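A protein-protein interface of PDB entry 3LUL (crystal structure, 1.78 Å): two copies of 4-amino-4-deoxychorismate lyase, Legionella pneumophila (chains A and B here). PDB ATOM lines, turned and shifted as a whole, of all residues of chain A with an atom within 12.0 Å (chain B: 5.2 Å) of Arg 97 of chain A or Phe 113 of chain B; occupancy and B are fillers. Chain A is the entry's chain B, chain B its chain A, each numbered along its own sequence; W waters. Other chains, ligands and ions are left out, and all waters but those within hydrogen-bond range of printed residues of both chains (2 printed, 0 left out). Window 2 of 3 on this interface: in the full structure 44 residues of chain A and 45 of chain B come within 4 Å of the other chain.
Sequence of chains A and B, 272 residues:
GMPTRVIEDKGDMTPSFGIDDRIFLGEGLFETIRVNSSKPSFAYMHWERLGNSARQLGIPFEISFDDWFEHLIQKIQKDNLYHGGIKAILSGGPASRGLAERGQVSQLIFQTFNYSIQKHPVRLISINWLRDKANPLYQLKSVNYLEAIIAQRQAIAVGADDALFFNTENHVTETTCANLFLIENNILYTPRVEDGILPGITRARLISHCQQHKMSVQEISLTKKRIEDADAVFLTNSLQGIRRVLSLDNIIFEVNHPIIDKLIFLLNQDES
No position is printed for both chains.
Of the 4 pairs that touch across the chains among the printed residues, none has its exchanged pair printed and touching as well.
Water W2 lies within hydrogen-bond range of NZ of Lys 87 of chain B and O of Phe 24 of chain A.
Water W1 bridges OG1 of Thr 32 of chain B (2.7 Å) and NH1 of Arg 97 of chain A (2.8 Å).
Arg 97 of chain A touches just these residues of chain B: Phe 113 (3.4 Å) and Leu 239 (3.2 Å).
Phe 113 of chain B touches just one residue of chain A: Arg 97.
No residue of chain A comes within 4 Å of Thr 32 of chain B.
Gly 85 of chain B touches none of the printed residues of chain A.
Of the printed residues of chain A, Lys 87 of chain B touches Leu 25.
No residue of chain A comes within 4 Å of Thr 112 of chain B.
No residue of chain A comes within 4 Å of Asn 114 of chain B.
No residue of chain A comes within 4 Å of Tyr 115 of chain B.
Printed residues of chain A within 4 Å of Leu 239 of chain B: Arg 97.
Printed residues of chain B within 4 Å of Ile 19 of chain A: Gln 111 (3.7 Å).
Of the printed residues of chain B, Leu 25 of chain A touches Lys 87 (3.5 Å).
Of the printed residues of chain A, Gln 111 of chain B touches Ile 19.
The nearest residue of chain B that does not touch Arg 97 of chain A is Tyr 115 of chain B (4.5 Å).
Hydrophobic or aromatic side chains of chain B that line the printed part of chain A: Phe 113 and Leu 239.
Along chain B the printed residues that touch a printed residue of chain A span positions 87 to 239.
Among the printed residues, no Asp or Glu carboxylate lies within 4 Å of a Lys or Arg side-chain nitrogen of the other chain.
Among the printed residues, pairs that only touch across the chains: Arg 97 of chain A with Leu 239 of chain B (3.2 Å), Arg 97 of chain A with Phe 113 of chain B (3.4 Å), Leu 25 of chain A with Lys 87 of chain B (3.5 Å) and Ile 19 of chain A with Gln 111 of chain B (3.7 Å).
O of Gln 111 of chain B sits at hydrogen-bond distance from N of Lys 87 of chain B (2.8 Å).
The backbone NH (N) of Gly 85 of chain B lies within hydrogen-bond range of the backbone carbonyl oxygen (O) of Phe 113 of chain B (2.9 Å).
The backbone carbonyl oxygen (O) of Leu 239 of chain B sits at hydrogen-bond distance from the side-chain hydroxyl (OH) of Tyr 115 of chain B.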
ATOM      1  N   GLY A  18      -8.857 -28.799 -37.762  1.00  0.00           N
ATOM      2  CA  GLY A  18     -10.090 -28.235 -37.204  1.00  0.00           C
ATOM      3  C   GLY A  18      -9.772 -27.658 -35.824  1.00  0.00           C
ATOM      4  O   GLY A  18      -8.761 -27.994 -35.219  1.00  0.00           O
ATOM      5  N   ILE A  19     -10.655 -26.813 -35.316  1.00  0.00           N
ATOM      6  CA  ILE A  19     -10.339 -26.037 -34.111  1.00  0.00           C
ATOM      7  C   ILE A  19     -10.316 -26.915 -32.853  1.00  0.00           C
ATOM      8  O   ILE A  19      -9.739 -26.536 -31.866  1.00  0.00           O
ATOM      9  CB  ILE A  19     -11.348 -24.887 -33.931  1.00  0.00           C
ATOM     10  CG1 ILE A  19     -10.806 -23.822 -32.959  1.00  0.00           C
ATOM     11  CG2 ILE A  19     -12.699 -25.437 -33.519  1.00  0.00           C
ATOM     12  CD1 ILE A  19      -9.488 -23.200 -33.405  1.00  0.00           C
ATOM     13  N   ASP A  20     -10.937 -28.083 -32.911  1.00  0.00           N
ATOM     14  CA  ASP A  20     -10.879 -29.073 -31.815  1.00  0.00           C
ATOM     15  C   ASP A  20      -9.621 -29.963 -31.821  1.00  0.00           C
ATOM     16  O   ASP A  20      -9.517 -30.885 -31.003  1.00  0.00           O
ATOM     17  CB  ASP A  20     -12.129 -29.964 -31.849  1.00  0.00           C
ATOM     18  CG  ASP A  20     -12.251 -30.779 -33.161  1.00  0.00           C
ATOM     19  OD1 ASP A  20     -11.560 -30.442 -34.160  1.00  0.00           O
ATOM     20  OD2 ASP A  20     -13.052 -31.748 -33.216  1.00  0.00           O
ATOM     21  N   ASP A  21      -8.697 -29.719 -32.765  1.00  0.00           N
ATOM     22  CA  ASP A  21      -7.478 -30.516 -32.893  1.00  0.00           C
ATOM     23  C   ASP A  21      -6.483 -30.155 -31.793  1.00  0.00           C
ATOM     24  O   ASP A  21      -6.308 -28.982 -31.435  1.00  0.00           O
ATOM     25  CB  ASP A  21      -6.855 -30.327 -34.291  1.00  0.00           C
ATOM     26  CG  ASP A  21      -5.876 -31.425 -34.656  1.00  0.00           C
ATOM     27  OD1 ASP A  21      -4.928 -31.627 -33.885  1.00  0.00           O
ATOM     28  OD2 ASP A  21      -6.055 -32.072 -35.712  1.00  0.00           O
ATOM     29  N   ARG A  22      -5.846 -31.176 -31.216  1.00  0.00           N
ATOM     30  CA  ARG A  22      -4.919 -30.932 -30.112  1.00  0.00           C
ATOM     31  C   ARG A  22      -3.636 -30.186 -30.555  1.00  0.00           C
ATOM     32  O   ARG A  22      -2.885 -29.696 -29.713  1.00  0.00           O
ATOM     33  CB  ARG A  22      -4.593 -32.235 -29.362  1.00  0.00           C
ATOM     34  CG  ARG A  22      -5.811 -32.847 -28.683  1.00  0.00           C
ATOM     35  CD  ARG A  22      -5.494 -34.134 -27.981  1.00  0.00           C
ATOM     36  NE  ARG A  22      -4.274 -34.051 -27.167  1.00  0.00           N
ATOM     37  CZ  ARG A  22      -4.198 -33.482 -25.954  1.00  0.00           C
ATOM     38  NH1 ARG A  22      -5.258 -32.944 -25.350  1.00  0.00           N
ATOM     39  NH2 ARG A  22      -3.043 -33.476 -25.320  1.00  0.00           N
ATOM     40  N   ILE A  23      -3.406 -30.058 -31.870  1.00  0.00           N
ATOM     41  CA  ILE A  23      -2.310 -29.235 -32.373  1.00  0.00           C
ATOM     42  C   ILE A  23      -2.393 -27.812 -31.839  1.00  0.00           C
ATOM     43  O   ILE A  23      -1.358 -27.160 -31.694  1.00  0.00           O
ATOM     44  CB  ILE A  23      -2.198 -29.288 -33.936  1.00  0.00           C
ATOM     45  CG1 ILE A  23      -0.878 -28.686 -34.436  1.00  0.00           C
ATOM     46  CG2 ILE A  23      -3.346 -28.571 -34.644  1.00  0.00           C
ATOM     47  CD1 ILE A  23      -0.558 -29.088 -35.898  1.00  0.00           C
ATOM     48  N   PHE A  24      -3.604 -27.317 -31.512  1.00  0.00           N
ATOM     49  CA  PHE A  24      -3.753 -25.986 -30.887  1.00  0.00           C
ATOM     50  C   PHE A  24      -3.315 -25.842 -29.425  1.00  0.00           C
ATOM     51  O   PHE A  24      -3.300 -24.747 -28.898  1.00  0.00           O
ATOM     52  CB  PHE A  24      -5.192 -25.473 -31.133  1.00  0.00           C
ATOM     53  CG  PHE A  24      -5.466 -25.212 -32.600  1.00  0.00           C
ATOM     54  CD1 PHE A  24      -4.850 -24.157 -33.238  1.00  0.00           C
ATOM     55  CD2 PHE A  24      -6.216 -26.054 -33.353  1.00  0.00           C
ATOM     56  CE1 PHE A  24      -5.054 -23.919 -34.599  1.00  0.00           C
ATOM     57  CE2 PHE A  24      -6.446 -25.809 -34.712  1.00  0.00           C
ATOM     58  CZ  PHE A  24      -5.838 -24.749 -35.329  1.00  0.00           C
ATOM     59  N   LEU A  25      -2.982 -26.971 -28.777  1.00  0.00           N
ATOM     60  CA  LEU A  25      -2.367 -27.035 -27.463  1.00  0.00           C
ATOM     61  C   LEU A  25      -0.859 -27.300 -27.590  1.00  0.00           C
ATOM     62  O   LEU A  25      -0.114 -27.402 -26.588  1.00  0.00           O
ATOM     63  CB  LEU A  25      -3.027 -28.178 -26.655  1.00  0.00           C
ATOM     64  CG  LEU A  25      -4.552 -28.221 -26.532  1.00  0.00           C
ATOM     65  CD1 LEU A  25      -5.040 -29.415 -25.718  1.00  0.00           C
ATOM     66  CD2 LEU A  25      -5.008 -26.927 -25.902  1.00  0.00           C
ATOM     67  N   GLU A  27       0.253 -30.040 -29.462  1.00  0.00           N
ATOM     68  CA  GLU A  27       0.442 -31.471 -29.685  1.00  0.00           C
ATOM     69  C   GLU A  27       0.538 -31.710 -31.191  1.00  0.00           C
ATOM     70  O   GLU A  27      -0.443 -32.062 -31.856  1.00  0.00           O
ATOM     71  CB  GLU A  27      -0.628 -32.356 -29.003  1.00  0.00           C
ATOM     72  CG  GLU A  27      -0.172 -33.801 -28.896  1.00  0.00           C
ATOM     73  CD  GLU A  27      -1.182 -34.628 -28.157  1.00  0.00           C
ATOM     74  OE1 GLU A  27      -2.232 -34.880 -28.747  1.00  0.00           O
ATOM     75  OE2 GLU A  27      -0.966 -34.954 -26.986  1.00  0.00           O
ATOM     76  N   GLY A  92      -1.998 -34.214 -33.134  1.00  0.00           N
ATOM     77  CA  GLY A  92      -2.581 -35.191 -32.199  1.00  0.00           C
ATOM     78  C   GLY A  92      -4.016 -35.520 -32.572  1.00  0.00           C
ATOM     79  O   GLY A  92      -4.516 -36.604 -32.285  1.00  0.00           O
ATOM     80  N   GLY A  93      -4.687 -34.596 -33.246  1.00  0.00           N
ATOM     81  CA  GLY A  93      -6.022 -34.839 -33.791  1.00  0.00           C
ATOM     82  C   GLY A  93      -7.154 -34.312 -32.933  1.00  0.00           C
ATOM     83  O   GLY A  93      -6.922 -33.849 -31.803  1.00  0.00           O
ATOM     84  N   PRO A  94      -8.406 -34.378 -33.467  1.00  0.00           N
ATOM     85  CA  PRO A  94      -9.584 -33.995 -32.710  1.00  0.00           C
ATOM     86  C   PRO A  94      -9.695 -34.815 -31.458  1.00  0.00           C
ATOM     87  O   PRO A  94      -9.435 -36.013 -31.476  1.00  0.00           O
ATOM     88  CB  PRO A  94     -10.757 -34.339 -33.637  1.00  0.00           C
ATOM     89  CG  PRO A  94     -10.214 -34.380 -34.974  1.00  0.00           C
ATOM     90  CD  PRO A  94      -8.733 -34.698 -34.870  1.00  0.00           C
ATOM     91  N   ALA A  95     -10.097 -34.180 -30.375  1.00  0.00           N
ATOM     92  CA  ALA A  95     -10.251 -34.886 -29.119  1.00  0.00           C
ATOM     93  C   ALA A  95     -11.169 -34.094 -28.240  1.00  0.00           C
ATOM     94  O   ALA A  95     -11.362 -32.890 -28.475  1.00  0.00           O
ATOM     95  CB  ALA A  95      -8.895 -35.046 -28.437  1.00  0.00           C
ATOM     96  N   SER A  96     -11.697 -34.748 -27.210  1.00  0.00           N
ATOM     97  CA  SER A  96     -12.479 -34.063 -26.183  1.00  0.00           C
ATOM     98  C   SER A  96     -11.571 -33.095 -25.459  1.00  0.00           C
ATOM     99  O   SER A  96     -10.331 -33.252 -25.461  1.00  0.00           O
ATOM    100  CB  SER A  96     -13.060 -35.043 -25.155  1.00  0.00           C
ATOM    101  OG  SER A  96     -14.165 -35.749 -25.664  1.00  0.00           O
ATOM    102  N   ARG A  97     -12.179 -32.105 -24.830  1.00  0.00           N
ATOM    103  CA  ARG A  97     -11.426 -31.082 -24.134  1.00  0.00           C
ATOM    104  C   ARG A  97     -10.691 -31.660 -22.918  1.00  0.00           C
ATOM    105  O   ARG A  97     -11.209 -32.525 -22.226  1.00  0.00           O
ATOM    106  CB  ARG A  97     -12.379 -29.971 -23.714  1.00  0.00           C
ATOM    107  CG  ARG A  97     -11.701 -28.750 -23.239  1.00  0.00           C
ATOM    108  CD  ARG A  97     -12.711 -27.742 -22.689  1.00  0.00           C
ATOM    109  NE  ARG A  97     -12.241 -27.251 -21.394  1.00  0.00           N
ATOM    110  CZ  ARG A  97     -11.237 -26.393 -21.210  1.00  0.00           C
ATOM    111  NH1 ARG A  97     -10.560 -25.874 -22.236  1.00  0.00           N
ATOM    112  NH2 ARG A  97     -10.909 -26.046 -19.972  1.00  0.00           N
ATOM    113  N   GLY A  98      -9.474 -31.173 -22.685  1.00  0.00           N
ATOM    114  CA  GLY A  98      -8.671 -31.573 -21.543  1.00  0.00           C
ATOM    115  C   GLY A  98      -7.222 -31.686 -21.944  1.00  0.00           C
ATOM    116  O   GLY A  98      -6.906 -32.228 -23.006  1.00  0.00           O
ATOM    117  N   LEU A  99      -6.332 -31.196 -21.096  1.00  0.00           N
ATOM    118  CA  LEU A  99      -4.917 -31.140 -21.443  1.00  0.00           C
ATOM    119  C   LEU A  99      -4.321 -32.534 -21.729  1.00  0.00           C
ATOM    120  O   LEU A  99      -3.472 -32.660 -22.599  1.00  0.00           O
ATOM    121  CB  LEU A  99      -4.130 -30.438 -20.337  1.00  0.00           C
ATOM    122  CG  LEU A  99      -2.746 -29.919 -20.636  1.00  0.00           C
ATOM    123  CD1 LEU A  99      -2.816 -28.804 -21.685  1.00  0.00           C
ATOM    124  CD2 LEU A  99      -2.038 -29.410 -19.352  1.00  0.00           C
ATOM    125  N   ALA A 100      -4.787 -33.558 -21.004  1.00  0.00           N
ATOM    126  CA  ALA A 100      -4.213 -34.913 -21.087  1.00  0.00           C
ATOM    127  C   ALA A 100      -5.119 -35.907 -21.827  1.00  0.00           C
ATOM    128  O   ALA A 100      -4.923 -37.133 -21.748  1.00  0.00           O
ATOM    129  CB  ALA A 100      -3.926 -35.439 -19.680  1.00  0.00           C
ATOM    130  N   GLU A 101      -6.122 -35.393 -22.523  1.00  0.00           N
ATOM    131  CA  GLU A 101      -6.908 -36.205 -23.426  1.00  0.00           C
ATOM    132  C   GLU A 101      -6.015 -36.702 -24.564  1.00  0.00           C
ATOM    133  O   GLU A 101      -4.899 -36.210 -24.772  1.00  0.00           O
ATOM    134  CB  GLU A 101      -8.096 -35.401 -23.983  1.00  0.00           C
ATOM    135  CG  GLU A 101      -9.110 -35.047 -22.901  1.00  0.00           C
ATOM    136  CD  GLU A 101      -9.769 -36.292 -22.318  1.00  0.00           C
ATOM    137  OE1 GLU A 101     -10.152 -37.167 -23.113  1.00  0.00           O
ATOM    138  OE2 GLU A 101      -9.890 -36.395 -21.082  1.00  0.00           O
ATOM    139  N   ARG A 102      -6.526 -37.667 -25.311  1.00  0.00           N
ATOM    140  CA  ARG A 102      -5.743 -38.372 -26.306  1.00  0.00           C
ATOM    141  C   ARG A 102      -6.552 -38.379 -27.610  1.00  0.00           C
ATOM    142  O   ARG A 102      -7.752 -38.712 -27.610  1.00  0.00           O
ATOM    143  CB  ARG A 102      -5.514 -39.785 -25.738  1.00  0.00           C
ATOM    144  CG  ARG A 102      -4.599 -40.719 -26.495  1.00  0.00           C
ATOM    145  CD  ARG A 102      -3.141 -40.571 -26.081  1.00  0.00           C
ATOM    146  NE  ARG A 102      -2.763 -41.149 -24.784  1.00  0.00           N
ATOM    147  CZ  ARG A 102      -1.529 -41.068 -24.255  1.00  0.00           C
ATOM    148  NH1 ARG A 102      -0.528 -40.441 -24.904  1.00  0.00           N
ATOM    149  NH2 ARG A 102      -1.279 -41.621 -23.071  1.00  0.00           N
ATOM    150  N   GLY A 103      -5.932 -37.988 -28.716  1.00  0.00           N
ATOM    151  CA  GLY A 103      -6.604 -38.061 -30.013  1.00  0.00           C
ATOM    152  C   GLY A 103      -6.546 -39.495 -30.468  1.00  0.00           C
ATOM    153  O   GLY A 103      -5.464 -40.081 -30.519  1.00  0.00           O
ATOM    154  N   GLN A 104      -7.702 -40.058 -30.783  1.00  0.00           N
ATOM    155  CA  GLN A 104      -7.784 -41.429 -31.288  1.00  0.00           C
ATOM    156  C   GLN A 104      -7.246 -41.519 -32.715  1.00  0.00           C
ATOM    157  O   GLN A 104      -6.717 -42.573 -33.103  1.00  0.00           O
ATOM    158  CB  GLN A 104      -9.238 -41.942 -31.304  1.00  0.00           C
ATOM    159  CG  GLN A 104     -10.059 -41.602 -30.060  1.00  0.00           C
ATOM    160  CD  GLN A 104     -10.845 -42.784 -29.522  1.00  0.00           C
ATOM    161  OE1 GLN A 104     -12.074 -42.861 -29.686  1.00  0.00           O
ATOM    162  NE2 GLN A 104     -10.139 -43.722 -28.883  1.00  0.00           N
ATOM    163  N   THR B  32      -8.800 -18.059 -21.405  1.00  0.00           N
ATOM    164  CA  THR B  32      -9.883 -18.937 -20.989  1.00  0.00           C
ATOM    165  C   THR B  32     -10.708 -18.192 -19.941  1.00  0.00           C
ATOM    166  O   THR B  32     -10.212 -17.902 -18.832  1.00  0.00           O
ATOM    167  CB  THR B  32      -9.329 -20.247 -20.411  1.00  0.00           C
ATOM    168  OG1 THR B  32      -8.592 -20.916 -21.432  1.00  0.00           O
ATOM    169  CG2 THR B  32     -10.452 -21.154 -19.988  1.00  0.00           C
ATOM    170  N   LEU B  81     -24.841 -20.767 -23.984  1.00  0.00           N
ATOM    171  CA  LEU B  81     -23.990 -20.985 -22.852  1.00  0.00           C
ATOM    172  C   LEU B  81     -24.540 -20.275 -21.628  1.00  0.00           C
ATOM    173  O   LEU B  81     -24.795 -19.074 -21.656  1.00  0.00           O
ATOM    174  CB  LEU B  81     -22.580 -20.511 -23.131  1.00  0.00           C
ATOM    175  CG  LEU B  81     -21.476 -20.897 -22.142  1.00  0.00           C
ATOM    176  CD1 LEU B  81     -21.214 -22.404 -22.145  1.00  0.00           C
ATOM    177  CD2 LEU B  81     -20.158 -20.139 -22.413  1.00  0.00           C
ATOM    178  N   HIS B  83     -23.612 -21.827 -17.906  1.00  0.00           N
ATOM    179  CA  HIS B  83     -22.417 -22.062 -17.098  1.00  0.00           C
ATOM    180  C   HIS B  83     -21.400 -22.780 -17.956  1.00  0.00           C
ATOM    181  O   HIS B  83     -21.686 -23.828 -18.540  1.00  0.00           O
ATOM    182  CB  HIS B  83     -22.699 -22.940 -15.854  1.00  0.00           C
ATOM    183  CG  HIS B  83     -23.602 -22.313 -14.831  1.00  0.00           C
ATOM    184  ND1 HIS B  83     -23.390 -21.044 -14.331  1.00  0.00           N
ATOM    185  CD2 HIS B  83     -24.704 -22.790 -14.189  1.00  0.00           C
ATOM    186  CE1 HIS B  83     -24.326 -20.759 -13.440  1.00  0.00           C
ATOM    187  NE2 HIS B  83     -25.126 -21.810 -13.317  1.00  0.00           N
ATOM    188  N   GLY B  84     -20.188 -22.250 -18.006  1.00  0.00           N
ATOM    189  CA  GLY B  84     -19.129 -22.919 -18.755  1.00  0.00           C
ATOM    190  C   GLY B  84     -18.005 -21.970 -19.022  1.00  0.00           C
ATOM    191  O   GLY B  84     -17.682 -21.143 -18.169  1.00  0.00           O
ATOM    192  N   GLY B  85     -17.407 -22.105 -20.187  1.00  0.00           N
ATOM    193  CA  GLY B  85     -16.247 -21.318 -20.520  1.00  0.00           C
ATOM    194  C   GLY B  85     -16.262 -20.857 -21.953  1.00  0.00           C
ATOM    195  O   GLY B  85     -16.972 -21.429 -22.823  1.00  0.00           O
ATOM    196  N   ILE B  86     -15.455 -19.812 -22.197  1.00  0.00           N
ATOM    197  CA  ILE B  86     -15.158 -19.316 -23.546  1.00  0.00           C
ATOM    198  C   ILE B  86     -13.637 -19.238 -23.707  1.00  0.00           C
ATOM    199  O   ILE B  86     -12.971 -18.621 -22.873  1.00  0.00           O
ATOM    200  CB  ILE B  86     -15.618 -17.871 -23.787  1.00  0.00           C
ATOM    201  CG1 ILE B  86     -17.137 -17.725 -23.784  1.00  0.00           C
ATOM    202  CG2 ILE B  86     -15.061 -17.384 -25.128  1.00  0.00           C
ATOM    203  CD1 ILE B  86     -17.607 -16.279 -24.024  1.00  0.00           C
ATOM    204  N   LYS B  87     -13.105 -19.853 -24.757  1.00  0.00           N
ATOM    205  CA  LYS B  87     -11.689 -19.770 -25.105  1.00  0.00           C
ATOM    206  C   LYS B  87     -11.546 -18.848 -26.302  1.00  0.00           C
ATOM    207  O   LYS B  87     -12.204 -19.049 -27.310  1.00  0.00           O
ATOM    208  CB  LYS B  87     -11.105 -21.160 -25.402  1.00  0.00           C
ATOM    209  CG  LYS B  87      -9.587 -21.160 -25.638  1.00  0.00           C
ATOM    210  CD  LYS B  87      -8.988 -22.549 -25.664  1.00  0.00           C
ATOM    211  CE  LYS B  87      -7.528 -22.545 -26.108  1.00  0.00           C
ATOM    212  NZ  LYS B  87      -6.859 -23.912 -26.004  1.00  0.00           N
ATOM    213  N   GLN B 111     -14.523 -19.808 -28.898  1.00  0.00           N
ATOM    214  CA  GLN B 111     -15.265 -21.089 -28.818  1.00  0.00           C
ATOM    215  C   GLN B 111     -15.779 -21.296 -27.412  1.00  0.00           C
ATOM    216  O   GLN B 111     -15.101 -20.942 -26.439  1.00  0.00           O
ATOM    217  CB  GLN B 111     -14.394 -22.289 -29.171  1.00  0.00           C
ATOM    218  CG  GLN B 111     -13.966 -22.337 -30.623  1.00  0.00           C
ATOM    219  CD  GLN B 111     -15.127 -22.697 -31.569  1.00  0.00           C
ATOM    220  OE1 GLN B 111     -15.699 -21.818 -32.271  1.00  0.00           O
ATOM    221  NE2 GLN B 111     -15.507 -23.986 -31.571  1.00  0.00           N
ATOM    222  N   THR B 112     -17.009 -21.781 -27.304  1.00  0.00           N
ATOM    223  CA  THR B 112     -17.570 -22.019 -25.963  1.00  0.00           C
ATOM    224  C   THR B 112     -17.443 -23.490 -25.662  1.00  0.00           C
ATOM    225  O   THR B 112     -17.298 -24.336 -26.579  1.00  0.00           O
ATOM    226  CB  THR B 112     -19.036 -21.597 -25.861  1.00  0.00           C
ATOM    227  OG1 THR B 112     -19.814 -22.387 -26.755  1.00  0.00           O
ATOM    228  CG2 THR B 112     -19.201 -20.098 -26.216  1.00  0.00           C
ATOM    229  N   PHE B 113     -17.588 -23.809 -24.388  1.00  0.00           N
ATOM    230  CA  PHE B 113     -17.534 -25.186 -23.933  1.00  0.00           C
ATOM    231  C   PHE B 113     -18.192 -25.303 -22.561  1.00  0.00           C
ATOM    232  O   PHE B 113     -18.189 -24.340 -21.794  1.00  0.00           O
ATOM    233  CB  PHE B 113     -16.088 -25.696 -23.900  1.00  0.00           C
ATOM    234  CG  PHE B 113     -15.177 -24.916 -23.038  1.00  0.00           C
ATOM    235  CD1 PHE B 113     -14.478 -23.812 -23.533  1.00  0.00           C
ATOM    236  CD2 PHE B 113     -14.990 -25.270 -21.706  1.00  0.00           C
ATOM    237  CE1 PHE B 113     -13.660 -23.088 -22.733  1.00  0.00           C
ATOM    238  CE2 PHE B 113     -14.152 -24.518 -20.877  1.00  0.00           C
ATOM    239  CZ  PHE B 113     -13.468 -23.445 -21.397  1.00  0.00           C
ATOM    240  N   ASN B 114     -18.769 -26.466 -22.291  1.00  0.00           N
ATOM    241  CA  ASN B 114     -19.113 -26.805 -20.916  1.00  0.00           C
ATOM    242  C   ASN B 114     -17.930 -27.465 -20.298  1.00  0.00           C
ATOM    243  O   ASN B 114     -17.082 -28.059 -21.010  1.00  0.00           O
ATOM    244  CB  ASN B 114     -20.305 -27.725 -20.876  1.00  0.00           C
ATOM    245  CG  ASN B 114     -21.546 -27.075 -21.427  1.00  0.00           C
ATOM    246  OD1 ASN B 114     -21.839 -25.927 -21.109  1.00  0.00           O
ATOM    247  ND2 ASN B 114     -22.303 -27.823 -22.234  1.00  0.00           N
ATOM    248  N   TYR B 115     -17.846 -27.387 -18.975  1.00  0.00           N
ATOM    249  CA  TYR B 115     -16.760 -28.081 -18.283  1.00  0.00           C
ATOM    250  C   TYR B 115     -17.212 -28.480 -16.895  1.00  0.00           C
ATOM    251  O   TYR B 115     -18.188 -27.953 -16.386  1.00  0.00           O
ATOM    252  CB  TYR B 115     -15.497 -27.230 -18.220  1.00  0.00           C
ATOM    253  CG  TYR B 115     -15.529 -26.110 -17.225  1.00  0.00           C
ATOM    254  CD1 TYR B 115     -16.084 -24.883 -17.539  1.00  0.00           C
ATOM    255  CD2 TYR B 115     -15.008 -26.286 -15.939  1.00  0.00           C
ATOM    256  CE1 TYR B 115     -16.118 -23.863 -16.624  1.00  0.00           C
ATOM    257  CE2 TYR B 115     -15.041 -25.251 -15.010  1.00  0.00           C
ATOM    258  CZ  TYR B 115     -15.581 -24.044 -15.366  1.00  0.00           C
ATOM    259  OH  TYR B 115     -15.621 -23.033 -14.462  1.00  0.00           O
ATOM    260  N   LEU B 239     -11.077 -21.281 -14.214  1.00  0.00           N
ATOM    261  CA  LEU B 239     -12.162 -22.241 -14.307  1.00  0.00           C
ATOM    262  C   LEU B 239     -12.463 -22.968 -13.020  1.00  0.00           C
ATOM    263  O   LEU B 239     -13.605 -23.245 -12.739  1.00  0.00           O
ATOM    264  CB  LEU B 239     -11.918 -23.242 -15.418  1.00  0.00           C
ATOM    265  CG  LEU B 239     -11.851 -22.614 -16.801  1.00  0.00           C
ATOM    266  CD1 LEU B 239     -11.645 -23.746 -17.832  1.00  0.00           C
ATOM    267  CD2 LEU B 239     -13.056 -21.786 -17.160  1.00  0.00           C
HETATM  268  O   HOH W   1      -9.065 -23.509 -22.194  1.00  0.00           O
HETATM  269  O   HOH W   2      -4.334 -23.351 -26.650  1.00  0.00           O
